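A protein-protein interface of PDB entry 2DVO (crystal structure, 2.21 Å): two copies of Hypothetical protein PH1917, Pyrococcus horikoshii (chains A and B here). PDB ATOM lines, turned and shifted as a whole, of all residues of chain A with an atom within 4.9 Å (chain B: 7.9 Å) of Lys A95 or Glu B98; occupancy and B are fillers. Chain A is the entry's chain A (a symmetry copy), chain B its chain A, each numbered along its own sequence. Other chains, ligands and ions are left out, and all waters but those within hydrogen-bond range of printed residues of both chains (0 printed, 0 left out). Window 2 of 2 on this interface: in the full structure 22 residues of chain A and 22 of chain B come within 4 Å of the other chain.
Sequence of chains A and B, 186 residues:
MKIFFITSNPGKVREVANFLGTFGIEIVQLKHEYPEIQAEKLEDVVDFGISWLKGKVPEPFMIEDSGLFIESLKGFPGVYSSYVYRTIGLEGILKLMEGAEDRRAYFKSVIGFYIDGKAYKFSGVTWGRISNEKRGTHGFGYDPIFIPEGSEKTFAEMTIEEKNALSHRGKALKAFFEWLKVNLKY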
ATOM      1  N   GLU A  91       1.083  17.312   4.076  1.00  0.00           N
ATOM      2  CA  GLU A  91       1.852  16.490   5.003  1.00  0.00           C
ATOM      3  C   GLU A  91       1.330  15.060   5.011  1.00  0.00           C
ATOM      4  O   GLU A  91       2.108  14.114   5.119  1.00  0.00           O
ATOM      5  CB  GLU A  91       1.826  17.092   6.412  1.00  0.00           C
ATOM      6  CG  GLU A  91       2.711  18.340   6.528  1.00  0.00           C
ATOM      7  CD  GLU A  91       4.210  18.026   6.467  1.00  0.00           C
ATOM      8  OE1 GLU A  91       4.582  16.972   5.900  1.00  0.00           O
ATOM      9  OE2 GLU A  91       5.016  18.839   6.978  1.00  0.00           O
ATOM     10  N   GLY A  92       0.015  14.906   4.872  1.00  0.00           N
ATOM     11  CA  GLY A  92      -0.576  13.581   4.855  1.00  0.00           C
ATOM     12  C   GLY A  92      -0.123  12.794   3.641  1.00  0.00           C
ATOM     13  O   GLY A  92       0.104  11.594   3.732  1.00  0.00           O
ATOM     14  N   ILE A  93       0.006  13.466   2.499  1.00  0.00           N
ATOM     15  CA  ILE A  93       0.454  12.805   1.276  1.00  0.00           C
ATOM     16  C   ILE A  93       1.913  12.376   1.439  1.00  0.00           C
ATOM     17  O   ILE A  93       2.272  11.233   1.149  1.00  0.00           O
ATOM     18  CB  ILE A  93       0.351  13.743   0.049  1.00  0.00           C
ATOM     19  CG1 ILE A  93      -1.103  14.178  -0.157  1.00  0.00           C
ATOM     20  CG2 ILE A  93       0.888  13.038  -1.200  1.00  0.00           C
ATOM     21  CD1 ILE A  93      -2.050  13.039  -0.524  1.00  0.00           C
ATOM     22  N   LEU A  94       2.752  13.297   1.904  1.00  0.00           N
ATOM     23  CA  LEU A  94       4.165  12.990   2.111  1.00  0.00           C
ATOM     24  C   LEU A  94       4.309  11.819   3.084  1.00  0.00           C
ATOM     25  O   LEU A  94       5.133  10.925   2.882  1.00  0.00           O
ATOM     26  CB  LEU A  94       4.906  14.217   2.658  1.00  0.00           C
ATOM     27  CG  LEU A  94       5.026  15.428   1.729  1.00  0.00           C
ATOM     28  CD1 LEU A  94       5.876  16.496   2.382  1.00  0.00           C
ATOM     29  CD2 LEU A  94       5.648  15.005   0.415  1.00  0.00           C
ATOM     30  N   LYS A  95       3.499  11.824   4.138  1.00  0.00           N
ATOM     31  CA  LYS A  95       3.528  10.753   5.128  1.00  0.00           C
ATOM     32  C   LYS A  95       3.255   9.413   4.447  1.00  0.00           C
ATOM     33  O   LYS A  95       3.981   8.436   4.652  1.00  0.00           O
ATOM     34  CB  LYS A  95       2.477  11.019   6.204  1.00  0.00           C
ATOM     35  CG  LYS A  95       2.381   9.950   7.281  1.00  0.00           C
ATOM     36  CD  LYS A  95       3.670   9.837   8.084  1.00  0.00           C
ATOM     37  CE  LYS A  95       3.447   8.987   9.329  1.00  0.00           C
ATOM     38  NZ  LYS A  95       2.370   9.579  10.175  1.00  0.00           N
ATOM     39  N   LEU A  96       2.212   9.381   3.623  1.00  0.00           N
ATOM     40  CA  LEU A  96       1.835   8.168   2.901  1.00  0.00           C
ATOM     41  C   LEU A  96       2.898   7.701   1.909  1.00  0.00           C
ATOM     42  O   LEU A  96       3.013   6.508   1.633  1.00  0.00           O
ATOM     43  CB  LEU A  96       0.507   8.386   2.157  1.00  0.00           C
ATOM     44  CG  LEU A  96      -0.771   8.441   3.006  1.00  0.00           C
ATOM     45  CD1 LEU A  96      -1.935   8.961   2.182  1.00  0.00           C
ATOM     46  CD2 LEU A  96      -1.079   7.052   3.543  1.00  0.00           C
ATOM     47  N   MET A  97       3.676   8.638   1.378  1.00  0.00           N
ATOM     48  CA  MET A  97       4.716   8.313   0.401  1.00  0.00           C
ATOM     49  C   MET A  97       6.092   7.996   1.004  1.00  0.00           C
ATOM     50  O   MET A  97       7.029   7.651   0.282  1.00  0.00           O
ATOM     51  CB  MET A  97       4.851   9.458  -0.607  1.00  0.00           C
ATOM     52  CG  MET A  97       3.606   9.687  -1.463  1.00  0.00           C
ATOM     53  SD  MET A  97       3.199   8.245  -2.462  1.00  0.00           S
ATOM     54  CE  MET A  97       4.259   8.536  -3.914  1.00  0.00           C
ATOM     55  N   GLU A  98       6.220   8.112   2.321  1.00  0.00           N
ATOM     56  CA  GLU A  98       7.491   7.817   2.978  1.00  0.00           C
ATOM     57  C   GLU A  98       7.966   6.412   2.625  1.00  0.00           C
ATOM     58  O   GLU A  98       7.249   5.431   2.838  1.00  0.00           O
ATOM     59  CB  GLU A  98       7.354   7.949   4.497  1.00  0.00           C
ATOM     60  CG  GLU A  98       7.480   9.379   5.014  1.00  0.00           C
ATOM     61  CD  GLU A  98       7.242   9.478   6.512  1.00  0.00           C
ATOM     62  OE1 GLU A  98       7.408   8.456   7.210  1.00  0.00           O
ATOM     63  OE2 GLU A  98       6.899  10.578   6.996  1.00  0.00           O
ATOM     64  N   SER B  72      -7.363  12.779  14.577  1.00  0.00           N
ATOM     65  CA  SER B  72      -6.041  13.277  14.219  1.00  0.00           C
ATOM     66  C   SER B  72      -5.883  13.570  12.726  1.00  0.00           C
ATOM     67  O   SER B  72      -4.933  14.242  12.322  1.00  0.00           O
ATOM     68  CB  SER B  72      -4.969  12.283  14.668  1.00  0.00           C
ATOM     69  OG  SER B  72      -5.257  10.987  14.182  1.00  0.00           O
ATOM     70  N   LEU B  73      -6.810  13.064  11.915  1.00  0.00           N
ATOM     71  CA  LEU B  73      -6.769  13.282  10.472  1.00  0.00           C
ATOM     72  C   LEU B  73      -7.863  14.262  10.066  1.00  0.00           C
ATOM     73  O   LEU B  73      -8.243  14.340   8.901  1.00  0.00           O
ATOM     74  CB  LEU B  73      -6.947  11.955   9.727  1.00  0.00           C
ATOM     75  CG  LEU B  73      -5.922  10.867  10.079  1.00  0.00           C
ATOM     76  CD1 LEU B  73      -6.182   9.627   9.246  1.00  0.00           C
ATOM     77  CD2 LEU B  73      -4.503  11.378   9.827  1.00  0.00           C
ATOM     78  N   GLU B  91      -3.843  -0.399   5.512  1.00  0.00           N
ATOM     79  CA  GLU B  91      -2.427  -0.095   5.686  1.00  0.00           C
ATOM     80  C   GLU B  91      -2.178   1.400   5.540  1.00  0.00           C
ATOM     81  O   GLU B  91      -1.343   1.964   6.245  1.00  0.00           O
ATOM     82  CB  GLU B  91      -1.575  -0.893   4.693  1.00  0.00           C
ATOM     83  CG  GLU B  91      -1.472  -2.375   5.074  1.00  0.00           C
ATOM     84  CD  GLU B  91      -0.616  -2.619   6.322  1.00  0.00           C
ATOM     85  OE1 GLU B  91      -0.474  -1.687   7.148  1.00  0.00           O
ATOM     86  OE2 GLU B  91      -0.093  -3.748   6.481  1.00  0.00           O
ATOM     87  N   GLY B  92      -2.922   2.042   4.643  1.00  0.00           N
ATOM     88  CA  GLY B  92      -2.766   3.471   4.440  1.00  0.00           C
ATOM     89  C   GLY B  92      -3.176   4.247   5.676  1.00  0.00           C
ATOM     90  O   GLY B  92      -2.552   5.247   6.014  1.00  0.00           O
ATOM     91  N   ILE B  93      -4.230   3.795   6.351  1.00  0.00           N
ATOM     92  CA  ILE B  93      -4.695   4.461   7.566  1.00  0.00           C
ATOM     93  C   ILE B  93      -3.646   4.294   8.666  1.00  0.00           C
ATOM     94  O   ILE B  93      -3.266   5.262   9.329  1.00  0.00           O
ATOM     95  CB  ILE B  93      -6.032   3.864   8.067  1.00  0.00           C
ATOM     96  CG1 ILE B  93      -7.114   4.031   6.996  1.00  0.00           C
ATOM     97  CG2 ILE B  93      -6.455   4.543   9.374  1.00  0.00           C
ATOM     98  CD1 ILE B  93      -7.482   5.482   6.700  1.00  0.00           C
ATOM     99  N   LEU B  94      -3.180   3.064   8.859  1.00  0.00           N
ATOM    100  CA  LEU B  94      -2.166   2.794   9.874  1.00  0.00           C
ATOM    101  C   LEU B  94      -0.918   3.636   9.604  1.00  0.00           C
ATOM    102  O   LEU B  94      -0.315   4.191  10.524  1.00  0.00           O
ATOM    103  CB  LEU B  94      -1.799   1.305   9.886  1.00  0.00           C
ATOM    104  CG  LEU B  94      -2.889   0.324  10.326  1.00  0.00           C
ATOM    105  CD1 LEU B  94      -2.326  -1.079  10.385  1.00  0.00           C
ATOM    106  CD2 LEU B  94      -3.419   0.725  11.687  1.00  0.00           C
ATOM    107  N   LYS B  95      -0.536   3.732   8.334  1.00  0.00           N
ATOM    108  CA  LYS B  95       0.629   4.519   7.945  1.00  0.00           C
ATOM    109  C   LYS B  95       0.447   5.967   8.397  1.00  0.00           C
ATOM    110  O   LYS B  95       1.341   6.560   9.008  1.00  0.00           O
ATOM    111  CB  LYS B  95       0.808   4.461   6.429  1.00  0.00           C
ATOM    112  CG  LYS B  95       1.973   5.276   5.891  1.00  0.00           C
ATOM    113  CD  LYS B  95       3.310   4.766   6.412  1.00  0.00           C
ATOM    114  CE  LYS B  95       4.457   5.397   5.632  1.00  0.00           C
ATOM    115  NZ  LYS B  95       4.327   5.092   4.178  1.00  0.00           N
ATOM    116  N   LEU B  96      -0.724   6.526   8.106  1.00  0.00           N
ATOM    117  CA  LEU B  96      -1.038   7.902   8.478  1.00  0.00           C
ATOM    118  C   LEU B  96      -1.073   8.124   9.990  1.00  0.00           C
ATOM    119  O   LEU B  96      -0.792   9.224  10.465  1.00  0.00           O
ATOM    120  CB  LEU B  96      -2.389   8.319   7.873  1.00  0.00           C
ATOM    121  CG  LEU B  96      -2.429   8.577   6.361  1.00  0.00           C
ATOM    122  CD1 LEU B  96      -3.863   8.674   5.876  1.00  0.00           C
ATOM    123  CD2 LEU B  96      -1.675   9.861   6.048  1.00  0.00           C
ATOM    124  N   MET B  97      -1.411   7.083  10.742  1.00  0.00           N
ATOM    125  CA  MET B  97      -1.496   7.182  12.200  1.00  0.00           C
ATOM    126  C   MET B  97      -0.193   6.864  12.946  1.00  0.00           C
ATOM    127  O   MET B  97      -0.131   6.971  14.172  1.00  0.00           O
ATOM    128  CB  MET B  97      -2.616   6.271  12.712  1.00  0.00           C
ATOM    129  CG  MET B  97      -4.012   6.669  12.238  1.00  0.00           C
ATOM    130  SD  MET B  97      -4.473   8.317  12.799  1.00  0.00           S
ATOM    131  CE  MET B  97      -5.137   7.931  14.451  1.00  0.00           C
ATOM    132  N   GLU B  98       0.845   6.471  12.217  1.00  0.00           N
ATOM    133  CA  GLU B  98       2.126   6.160  12.846  1.00  0.00           C
ATOM    134  C   GLU B  98       2.614   7.336  13.684  1.00  0.00           C
ATOM    135  O   GLU B  98       2.756   8.454  13.181  1.00  0.00           O
ATOM    136  CB  GLU B  98       3.175   5.812  11.786  1.00  0.00           C
ATOM    137  CG  GLU B  98       3.121   4.364  11.305  1.00  0.00           C
ATOM    138  CD  GLU B  98       4.112   4.086  10.187  1.00  0.00           C
ATOM    139  OE1 GLU B  98       5.106   4.834  10.074  1.00  0.00           O
ATOM    140  OE2 GLU B  98       3.905   3.118   9.425  1.00  0.00           O
ATOM    141  N   GLY B  99       2.855   7.078  14.967  1.00  0.00           N
ATOM    142  CA  GLY B  99       3.328   8.122  15.859  1.00  0.00           C
ATOM    143  C   GLY B  99       2.216   9.014  16.377  1.00  0.00           C
ATOM    144  O   GLY B  99       2.462   9.959  17.125  1.00  0.00           O
ATOM    145  N   ALA B 100       0.983   8.721  15.977  1.00  0.00           N
ATOM    146  CA  ALA B 100      -0.150   9.517  16.419  1.00  0.00           C
ATOM    147  C   ALA B 100      -0.431   9.275  17.897  1.00  0.00           C
ATOM    148  O   ALA B 100      -0.555   8.134  18.341  1.00  0.00           O
ATOM    149  CB  ALA B 100      -1.385   9.175  15.589  1.00  0.00           C
ATOM    150  N   GLU B 101      -0.517  10.364  18.649  1.00  0.00           N
ATOM    151  CA  GLU B 101      -0.807  10.309  20.073  1.00  0.00           C
ATOM    152  C   GLU B 101      -2.273   9.944  20.220  1.00  0.00           C
ATOM    153  O   GLU B 101      -2.622   8.916  20.809  1.00  0.00           O
ATOM    154  CB  GLU B 101      -0.571  11.682  20.703  1.00  0.00           C
ATOM    155  CG  GLU B 101      -1.286  12.821  19.975  1.00  0.00           C
ATOM    156  CD  GLU B 101      -2.058  13.730  20.922  1.00  0.00           C
ATOM    157  OE1 GLU B 101      -3.088  13.298  21.479  1.00  0.00           O
ATOM    158  OE2 GLU B 101      -1.631  14.884  21.113  1.00  0.00           O
ATOM    159  N   ARG B 103      -5.421   8.546  18.896  1.00  0.00           N
ATOM    160  CA  ARG B 103      -5.883   7.599  17.892  1.00  0.00           C
ATOM    161  C   ARG B 103      -7.409   7.510  17.910  1.00  0.00           C
ATOM    162  O   ARG B 103      -8.005   6.629  17.277  1.00  0.00           O
ATOM    163  CB  ARG B 103      -5.267   6.213  18.132  1.00  0.00           C
ATOM    164  CG  ARG B 103      -3.732   6.203  18.174  1.00  0.00           C
ATOM    165  CD  ARG B 103      -3.168   4.778  18.249  1.00  0.00           C
ATOM    166  NE  ARG B 103      -3.319   4.040  16.994  1.00  0.00           N
ATOM    167  CZ  ARG B 103      -2.483   4.127  15.960  1.00  0.00           C
ATOM    168  NH1 ARG B 103      -1.418   4.918  16.018  1.00  0.00           N
ATOM    169  NH2 ARG B 103      -2.713   3.422  14.859  1.00  0.00           N
ATOM    170  N   ASN B 132      -3.254  -0.423  16.330  1.00  0.00           N
ATOM    171  CA  ASN B 132      -1.945  -0.321  15.694  1.00  0.00           C
ATOM    172  C   ASN B 132      -1.794  -1.524  14.767  1.00  0.00           C
ATOM    173  O   ASN B 132      -0.998  -1.498  13.830  1.00  0.00           O
ATOM    174  CB  ASN B 132      -0.837  -0.305  16.750  1.00  0.00           C
ATOM    175  CG  ASN B 132      -0.751   1.027  17.483  1.00  0.00           C
ATOM    176  OD1 ASN B 132      -0.166   1.989  16.983  1.00  0.00           O
ATOM    177  ND2 ASN B 132      -1.355   1.093  18.662  1.00  0.00           N
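The side-chain amino group (NZ) of Lys B95 lies within hydrogen-bond range of the backbone carbonyl oxygen (O) of Glu A98 (3.2 Å).
The backbone carbonyl oxygen (O) of Lys A95 sits close to the side-chain amino group (NZ) of Lys B95 (3.4 Å).
The backbone carbonyl oxygen (O) of Leu A96 lies within hydrogen-bond range of the side-chain amino group (NZ) of Lys B95.
NZ of Lys A95 lies within hydrogen-bond range of O of Leu B96 (3.2 Å).
O of Glu B98 is in hydrogen-bond range of NZ of Lys A95.
O of Gly A92 touches CD2 of Leu B96 (3.4 Å).
O of Gly B92 touches CD2 of Leu A96 (3.4 Å).
Leu A96 touches Leu B96 (CG to CD2, 3.5 Å).
Of chain B, only Lys B95 (3.2 Å), Leu B96 (3.2 Å) and Glu B98 (3.2 Å) come within 4 Å of Lys A95.
Of chain A, only Lys A95 comes within 4 Å of Glu B98.
Printed residues of chain B within 4 Å of Gly A92: Leu B96.
Printed residues of chain A within 4 Å of Leu B96: Gly A92, Lys A95 and Leu A96.
Glu B91 touches none of the printed residues of chain A.
Gly B99 touches none of the printed residues of chain A.
The nearest printed residue of chain B that does not touch Leu A96 is Ile B93 (5.3 Å).
Hydrophobic or aromatic side chains of chain A that line the printed part of chain B: Leu A96.
Of the 15 printed residues of chain B, 4 touch a printed residue of chain A.
Hydrophobic or aromatic side chains of chain B within 4 Å of the printed part of chain A: Leu B96.
Among the printed residues, 8 pairs touch across the chains.
Among the printed residues, no Asp or Glu carboxylate lies within 4 Å of a Lys or Arg side-chain nitrogen of the other chain.
Lys B95 touches its own counterpart, Lys A95.
Lys A95 touches Leu B96, and with the chains exchanged Leu A96 touches Lys B95.
Lys A95 touches Glu B98, and with the chains exchanged Glu A98 touches Lys B95.
Leu B96 touches its own counterpart, Leu A96.
8 positions are printed for both chains.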
